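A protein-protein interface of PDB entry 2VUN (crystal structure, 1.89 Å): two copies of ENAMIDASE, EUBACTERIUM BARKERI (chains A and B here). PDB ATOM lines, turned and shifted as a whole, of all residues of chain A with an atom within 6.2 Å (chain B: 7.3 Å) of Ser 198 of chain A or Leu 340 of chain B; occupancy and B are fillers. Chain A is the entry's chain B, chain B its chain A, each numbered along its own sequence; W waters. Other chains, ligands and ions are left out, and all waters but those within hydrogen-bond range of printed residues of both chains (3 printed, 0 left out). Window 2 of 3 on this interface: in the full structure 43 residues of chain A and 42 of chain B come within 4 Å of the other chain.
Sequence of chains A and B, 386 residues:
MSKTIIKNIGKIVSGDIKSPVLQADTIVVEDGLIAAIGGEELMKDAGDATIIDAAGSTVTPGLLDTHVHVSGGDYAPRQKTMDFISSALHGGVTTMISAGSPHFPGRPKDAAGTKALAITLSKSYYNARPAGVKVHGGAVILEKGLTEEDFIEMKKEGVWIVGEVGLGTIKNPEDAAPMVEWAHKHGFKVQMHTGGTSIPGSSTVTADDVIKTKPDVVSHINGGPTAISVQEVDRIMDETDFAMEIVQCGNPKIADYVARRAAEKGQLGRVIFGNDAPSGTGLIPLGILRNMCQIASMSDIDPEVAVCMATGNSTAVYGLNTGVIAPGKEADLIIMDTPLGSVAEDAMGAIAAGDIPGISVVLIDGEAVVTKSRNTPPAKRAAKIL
No position is printed for both chains. Of the 9 pairs that touch across the chains among the printed residues, none has its exchanged pair printed and touching as well.
Printed residues of chain B that touch a printed residue of chain A: Pro 339, Leu 340, Gly 341, Ser 342, Asp 355 and Pro 377. Hydrophobic or aromatic side chains of chain B that line the printed part of chain A: Pro 339, Leu 340 and Pro 377. Of the 10 printed residues of chain A, 5 touch a printed residue of chain B. Printed residues of chain A that touch a printed residue of chain B: Gly 196, Thr 197, Ser 198, Ser 203 and Thr 226. Among the printed residues, 9 pairs touch across the chains. Among the printed residues, no Asp or Glu carboxylate lies within 4 Å of a Lys or Arg side-chain nitrogen of the other chain.
Of chain B, only Leu 340 (3.7 Å) comes within 4 Å of Ser 198 of chain A. Printed residues of chain A within 4 Å of Leu 340 of chain B: Gly 196, Thr 197, Ser 198 and Thr 226. Of the printed residues of chain A, Gly 341 of chain B touches Ser 203. Printed residues of chain A within 4 Å of Ser 342 of chain B: Thr 226 (3.6 Å). Pro 200 of chain A touches none of the printed residues of chain B. Lys 372 of chain B touches none of the printed residues of chain A. The nearest printed residue of chain A that does not touch Leu 340 of chain B is Pro 200 of chain A (4.01 Å). The nearest printed residue of chain B that does not touch Thr 197 of chain A is Pro 378 of chain B (4.2 Å).
Water W1 lies within hydrogen-bond range of OG1 of Thr 204 of chain A (2.7 Å), O of Gly 341 of chain B (2.7 Å) and N of Gly 196 of chain A (3.3 Å). Water W3 bridges O of Leu 340 of chain B (2.7 Å) and OG1 of Thr 226 of chain A (2.9 Å). Water W2 bridges the backbone carbonyl oxygen of Ile 356 of chain B (2.8 Å) and the side-chain hydroxyl of Thr 226 of chain A (2.8 Å).
OG of Ser 342 of chain B sits at hydrogen-bond distance from OD2 of Asp 355 of chain B (2.8 Å). The backbone NH (N) of Leu 340 of chain B is in hydrogen-bond range of the backbone carbonyl oxygen (O) of Pro 378 of chain B (3.0 Å). The backbone NH (N) of Gly 196 of chain A is in hydrogen-bond range of the backbone carbonyl oxygen (O) of Thr 226 of chain A (3.0 Å). The side-chain hydroxyl of Thr 197 of chain A is in hydrogen-bond range of the backbone carbonyl oxygen of Ser 202 of chain A (2.6 Å). The backbone NH of Thr 197 of chain A is in hydrogen-bond range of the backbone carbonyl oxygen of Ser 203 of chain A, at 2.8 Å.
Among the printed residues, merely in contact across the chains: Ser 203 of chain A with Gly 341 of chain B (3.2 Å), Thr 197 of chain A with Leu 340 of chain B (3.3 Å), Thr 226 of chain A with Pro 339 of chain B (3.6 Å), Thr 226 of chain A with Ser 342 of chain B (3.6 Å), Thr 226 of chain A with Asp 355 of chain B (3.7 Å), Gly 196 of chain A with Leu 340 of chain B (3.7 Å), Thr 226 of chain A with Leu 340 of chain B (3.7 Å), Ser 198 of chain A with Leu 340 of chain B (3.7 Å) and Thr 226 of chain A with Pro 377 of chain B (3.8 Å).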
ATOM      1  N   GLY A 195       7.977  21.923  12.296  1.00  0.00           N
ATOM      2  CA  GLY A 195       7.355  21.562  11.034  1.00  0.00           C
ATOM      3  C   GLY A 195       7.492  20.079  10.790  1.00  0.00           C
ATOM      4  O   GLY A 195       7.787  19.315  11.718  1.00  0.00           O
ATOM      5  N   GLY A 196       7.285  19.682   9.535  1.00  0.00           N
ATOM      6  CA  GLY A 196       7.351  18.282   9.133  1.00  0.00           C
ATOM      7  C   GLY A 196       8.687  17.651   9.463  1.00  0.00           C
ATOM      8  O   GLY A 196       9.733  18.303   9.352  1.00  0.00           O
ATOM      9  N   THR A 197       8.644  16.389   9.886  1.00  0.00           N
ATOM     10  CA  THR A 197       9.846  15.634  10.247  1.00  0.00           C
ATOM     11  C   THR A 197      10.028  14.430   9.320  1.00  0.00           C
ATOM     12  O   THR A 197       9.217  14.205   8.419  1.00  0.00           O
ATOM     13  CB  THR A 197       9.817  15.157  11.731  1.00  0.00           C
ATOM     14  OG1 THR A 197       8.720  14.256  11.933  1.00  0.00           O
ATOM     15  CG2 THR A 197       9.688  16.338  12.689  1.00  0.00           C
ATOM     16  N   SER A 198      11.095  13.665   9.541  1.00  0.00           N
ATOM     17  CA  SER A 198      11.389  12.487   8.724  1.00  0.00           C
ATOM     18  C   SER A 198      10.898  11.188   9.382  1.00  0.00           C
ATOM     19  O   SER A 198      11.120  10.090   8.861  1.00  0.00           O
ATOM     20  CB  SER A 198      12.891  12.413   8.428  1.00  0.00           C
ATOM     21  OG  SER A 198      13.340  13.607   7.807  1.00  0.00           O
ATOM     22  N   ILE A 199      10.218  11.328  10.516  1.00  0.00           N
ATOM     23  CA  ILE A 199       9.689  10.186  11.257  1.00  0.00           C
ATOM     24  C   ILE A 199       8.190  10.022  10.971  1.00  0.00           C
ATOM     25  O   ILE A 199       7.391  10.891  11.333  1.00  0.00           O
ATOM     26  CB  ILE A 199       9.950  10.312  12.792  1.00  0.00           C
ATOM     27  CG1 ILE A 199      11.454  10.272  13.103  1.00  0.00           C
ATOM     28  CG2 ILE A 199       9.242   9.199  13.564  1.00  0.00           C
ATOM     29  CD1 ILE A 199      12.168  11.616  13.008  1.00  0.00           C
ATOM     30  N   PRO A 200       7.810   8.915  10.299  1.00  0.00           N
ATOM     31  CA  PRO A 200       6.400   8.607  10.025  1.00  0.00           C
ATOM     32  C   PRO A 200       5.515   8.583  11.282  1.00  0.00           C
ATOM     33  O   PRO A 200       4.355   9.006  11.217  1.00  0.00           O
ATOM     34  CB  PRO A 200       6.466   7.221   9.377  1.00  0.00           C
ATOM     35  CG  PRO A 200       7.822   7.174   8.757  1.00  0.00           C
ATOM     36  CD  PRO A 200       8.708   7.896   9.724  1.00  0.00           C
ATOM     37  N   SER A 202       5.910  10.266  14.523  1.00  0.00           N
ATOM     38  CA  SER A 202       5.669  11.668  14.882  1.00  0.00           C
ATOM     39  C   SER A 202       6.135  12.565  13.734  1.00  0.00           C
ATOM     40  O   SER A 202       7.293  12.995  13.688  1.00  0.00           O
ATOM     41  CB  SER A 202       6.365  12.032  16.202  1.00  0.00           C
ATOM     42  OG  SER A 202       7.732  11.647  16.194  1.00  0.00           O
ATOM     43  N   SER A 203       5.216  12.829  12.807  1.00  0.00           N
ATOM     44  CA  SER A 203       5.541  13.469  11.529  1.00  0.00           C
ATOM     45  C   SER A 203       5.614  14.997  11.583  1.00  0.00           C
ATOM     46  O   SER A 203       6.089  15.632  10.636  1.00  0.00           O
ATOM     47  CB  SER A 203       4.555  13.016  10.447  1.00  0.00           C
ATOM     48  OG  SER A 203       3.223  13.362  10.797  1.00  0.00           O
ATOM     49  N   THR A 204       5.158  15.578  12.691  1.00  0.00           N
ATOM     50  CA  THR A 204       5.099  17.032  12.844  1.00  0.00           C
ATOM     51  C   THR A 204       5.422  17.492  14.274  1.00  0.00           C
ATOM     52  O   THR A 204       5.506  16.680  15.197  1.00  0.00           O
ATOM     53  CB  THR A 204       3.726  17.598  12.377  1.00  0.00           C
ATOM     54  OG1 THR A 204       3.749  19.033  12.408  1.00  0.00           O
ATOM     55  CG2 THR A 204       2.573  17.076  13.253  1.00  0.00           C
ATOM     56  N   THR A 226       8.533  21.816   5.073  1.00  0.00           N
ATOM     57  CA  THR A 226       7.138  21.435   5.341  1.00  0.00           C
ATOM     58  C   THR A 226       6.573  22.132   6.579  1.00  0.00           C
ATOM     59  O   THR A 226       7.104  21.980   7.682  1.00  0.00           O
ATOM     60  CB  THR A 226       7.010  19.906   5.506  1.00  0.00           C
ATOM     61  OG1 THR A 226       7.573  19.263   4.358  1.00  0.00           O
ATOM     62  CG2 THR A 226       5.544  19.486   5.651  1.00  0.00           C
ATOM     63  N   ASP B 337       4.376  12.576  -3.633  1.00  0.00           N
ATOM     64  CA  ASP B 337       3.317  12.535  -2.647  1.00  0.00           C
ATOM     65  C   ASP B 337       3.376  13.775  -1.766  1.00  0.00           C
ATOM     66  O   ASP B 337       4.337  14.551  -1.810  1.00  0.00           O
ATOM     67  CB  ASP B 337       3.438  11.259  -1.789  1.00  0.00           C
ATOM     68  CG  ASP B 337       2.125  10.877  -1.093  1.00  0.00           C
ATOM     69  OD1 ASP B 337       1.052  11.397  -1.467  1.00  0.00           O
ATOM     70  OD2 ASP B 337       2.177  10.047  -0.161  1.00  0.00           O
ATOM     71  N   THR B 338       2.323  13.970  -0.987  1.00  0.00           N
ATOM     72  CA  THR B 338       2.389  14.873   0.138  1.00  0.00           C
ATOM     73  C   THR B 338       3.597  14.465   0.987  1.00  0.00           C
ATOM     74  O   THR B 338       3.878  13.267   1.128  1.00  0.00           O
ATOM     75  CB  THR B 338       1.080  14.841   0.953  1.00  0.00           C
ATOM     76  OG1 THR B 338       1.140  15.832   1.982  1.00  0.00           O
ATOM     77  CG2 THR B 338       0.816  13.454   1.563  1.00  0.00           C
ATOM     78  N   PRO B 339       4.342  15.451   1.517  1.00  0.00           N
ATOM     79  CA  PRO B 339       5.508  15.125   2.337  1.00  0.00           C
ATOM     80  C   PRO B 339       5.085  14.826   3.774  1.00  0.00           C
ATOM     81  O   PRO B 339       4.019  15.259   4.204  1.00  0.00           O
ATOM     82  CB  PRO B 339       6.334  16.414   2.284  1.00  0.00           C
ATOM     83  CG  PRO B 339       5.283  17.506   2.186  1.00  0.00           C
ATOM     84  CD  PRO B 339       4.148  16.912   1.382  1.00  0.00           C
ATOM     85  N   LEU B 340       5.917  14.086   4.500  1.00  0.00           N
ATOM     86  CA  LEU B 340       5.627  13.740   5.889  1.00  0.00           C
ATOM     87  C   LEU B 340       5.326  14.997   6.695  1.00  0.00           C
ATOM     88  O   LEU B 340       6.057  15.979   6.608  1.00  0.00           O
ATOM     89  CB  LEU B 340       6.804  12.978   6.514  1.00  0.00           C
ATOM     90  CG  LEU B 340       6.915  11.490   6.183  1.00  0.00           C
ATOM     91  CD1 LEU B 340       8.151  10.902   6.835  1.00  0.00           C
ATOM     92  CD2 LEU B 340       5.660  10.731   6.631  1.00  0.00           C
ATOM     93  N   GLY B 341       4.227  14.967   7.441  1.00  0.00           N
ATOM     94  CA  GLY B 341       3.862  16.070   8.326  1.00  0.00           C
ATOM     95  C   GLY B 341       3.014  17.170   7.710  1.00  0.00           C
ATOM     96  O   GLY B 341       2.514  18.036   8.428  1.00  0.00           O
ATOM     97  N   SER B 342       2.842  17.151   6.391  1.00  0.00           N
ATOM     98  CA  SER B 342       2.017  18.167   5.727  1.00  0.00           C
ATOM     99  C   SER B 342       0.538  18.032   6.094  1.00  0.00           C
ATOM    100  O   SER B 342       0.041  16.925   6.291  1.00  0.00           O
ATOM    101  CB  SER B 342       2.169  18.081   4.208  1.00  0.00           C
ATOM    102  OG  SER B 342       1.275  18.982   3.563  1.00  0.00           O
ATOM    103  N   VAL B 343      -0.161  19.163   6.158  1.00  0.00           N
ATOM    104  CA  VAL B 343      -1.619  19.170   6.360  1.00  0.00           C
ATOM    105  C   VAL B 343      -2.355  18.502   5.197  1.00  0.00           C
ATOM    106  O   VAL B 343      -3.479  18.012   5.357  1.00  0.00           O
ATOM    107  CB  VAL B 343      -2.186  20.607   6.576  1.00  0.00           C
ATOM    108  CG1 VAL B 343      -1.612  21.228   7.836  1.00  0.00           C
ATOM    109  CG2 VAL B 343      -1.944  21.519   5.353  1.00  0.00           C
ATOM    110  N   ASP B 355       3.423  23.561   0.384  1.00  0.00           N
ATOM    111  CA  ASP B 355       4.446  22.586   0.792  1.00  0.00           C
ATOM    112  C   ASP B 355       5.039  21.901  -0.433  1.00  0.00           C
ATOM    113  O   ASP B 355       4.301  21.382  -1.268  1.00  0.00           O
ATOM    114  CB  ASP B 355       3.839  21.502   1.700  1.00  0.00           C
ATOM    115  CG  ASP B 355       3.553  21.985   3.123  1.00  0.00           C
ATOM    116  OD1 ASP B 355       4.250  22.887   3.644  1.00  0.00           O
ATOM    117  OD2 ASP B 355       2.616  21.428   3.732  1.00  0.00           O
ATOM    118  N   ILE B 356       6.368  21.894  -0.539  1.00  0.00           N
ATOM    119  CA  ILE B 356       7.050  21.144  -1.588  1.00  0.00           C
ATOM    120  C   ILE B 356       6.695  19.660  -1.419  1.00  0.00           C
ATOM    121  O   ILE B 356       6.824  19.132  -0.315  1.00  0.00           O
ATOM    122  CB  ILE B 356       8.605  21.326  -1.519  1.00  0.00           C
ATOM    123  CG1 ILE B 356       8.987  22.796  -1.731  1.00  0.00           C
ATOM    124  CG2 ILE B 356       9.300  20.424  -2.545  1.00  0.00           C
ATOM    125  CD1 ILE B 356      10.488  23.072  -1.677  1.00  0.00           C
ATOM    126  N   GLY B 358       7.048  15.512  -1.742  1.00  0.00           N
ATOM    127  CA  GLY B 358       8.142  14.543  -1.716  1.00  0.00           C
ATOM    128  C   GLY B 358       8.189  13.755  -3.007  1.00  0.00           C
ATOM    129  O   GLY B 358       7.191  13.198  -3.433  1.00  0.00           O
ATOM    130  N   LYS B 372      14.716   7.738  -4.822  1.00  0.00           N
ATOM    131  CA  LYS B 372      14.325   8.551  -3.682  1.00  0.00           C
ATOM    132  C   LYS B 372      15.020   9.903  -3.834  1.00  0.00           C
ATOM    133  O   LYS B 372      16.250   9.962  -4.019  1.00  0.00           O
ATOM    134  CB  LYS B 372      14.710   7.902  -2.349  1.00  0.00           C
ATOM    135  CG  LYS B 372      14.274   8.727  -1.150  1.00  0.00           C
ATOM    136  CD  LYS B 372      14.649   8.068   0.167  1.00  0.00           C
ATOM    137  CE  LYS B 372      14.218   8.948   1.327  1.00  0.00           C
ATOM    138  NZ  LYS B 372      14.191   8.211   2.632  1.00  0.00           N
ATOM    139  N   PRO B 377      11.628  17.003   0.724  1.00  0.00           N
ATOM    140  CA  PRO B 377      11.262  16.304   1.957  1.00  0.00           C
ATOM    141  C   PRO B 377      10.783  14.890   1.600  1.00  0.00           C
ATOM    142  O   PRO B 377      10.517  14.617   0.427  1.00  0.00           O
ATOM    143  CB  PRO B 377      10.120  17.161   2.527  1.00  0.00           C
ATOM    144  CG  PRO B 377       9.622  18.003   1.356  1.00  0.00           C
ATOM    145  CD  PRO B 377      10.842  18.241   0.529  1.00  0.00           C
ATOM    146  N   PRO B 378      10.704  13.980   2.583  1.00  0.00           N
ATOM    147  CA  PRO B 378      10.291  12.611   2.265  1.00  0.00           C
ATOM    148  C   PRO B 378       8.811  12.487   1.904  1.00  0.00           C
ATOM    149  O   PRO B 378       7.964  13.017   2.615  1.00  0.00           O
ATOM    150  CB  PRO B 378      10.582  11.845   3.562  1.00  0.00           C
ATOM    151  CG  PRO B 378      10.568  12.887   4.638  1.00  0.00           C
ATOM    152  CD  PRO B 378      11.026  14.157   4.014  1.00  0.00           C
ATOM    153  N   ALA B 379       8.512  11.803   0.800  1.00  0.00           N
ATOM    154  CA  ALA B 379       7.133  11.472   0.449  1.00  0.00           C
ATOM    155  C   ALA B 379       6.513  10.600   1.538  1.00  0.00           C
ATOM    156  O   ALA B 379       7.171   9.703   2.068  1.00  0.00           O
ATOM    157  CB  ALA B 379       7.091  10.756  -0.878  1.00  0.00           C
ATOM    158  N   LYS B 380       5.252  10.864   1.873  1.00  0.00           N
ATOM    159  CA  LYS B 380       4.519  10.042   2.844  1.00  0.00           C
ATOM    160  C   LYS B 380       4.427   8.598   2.339  1.00  0.00           C
ATOM    161  O   LYS B 380       4.711   7.653   3.077  1.00  0.00           O
ATOM    162  CB  LYS B 380       3.122  10.624   3.097  1.00  0.00           C
ATOM    163  CG  LYS B 380       2.278   9.851   4.126  1.00  0.00           C
ATOM    164  CD  LYS B 380       0.897  10.507   4.344  1.00  0.00           C
ATOM    165  CE  LYS B 380      -0.169   9.968   3.388  1.00  0.00           C
ATOM    166  NZ  LYS B 380      -1.471  10.749   3.422  1.00  0.00           N
ATOM    167  N   ARG B 381       4.032   8.448   1.077  1.00  0.00           N
ATOM    168  CA  ARG B 381       3.938   7.149   0.419  1.00  0.00           C
ATOM    169  C   ARG B 381       4.930   7.123  -0.736  1.00  0.00           C
ATOM    170  O   ARG B 381       4.771   7.854  -1.714  1.00  0.00           O
ATOM    171  CB  ARG B 381       2.513   6.906  -0.089  1.00  0.00           C
ATOM    172  CG  ARG B 381       1.483   6.792   1.035  1.00  0.00           C
ATOM    173  CD  ARG B 381       0.068   6.989   0.527  1.00  0.00           C
ATOM    174  NE  ARG B 381      -0.155   8.366   0.085  1.00  0.00           N
ATOM    175  CZ  ARG B 381      -1.342   8.859  -0.264  1.00  0.00           C
ATOM    176  NH1 ARG B 381      -2.426   8.094  -0.217  1.00  0.00           N
ATOM    177  NH2 ARG B 381      -1.450  10.122  -0.657  1.00  0.00           N
HETATM  178  O   HOH W   1       3.979  19.780   9.847  1.00  0.00           O
HETATM  179  O   HOH W   2       7.265  20.608   1.968  1.00  0.00           O
HETATM  180  O   HOH W   3       8.380  16.698   5.480  1.00  0.00           O
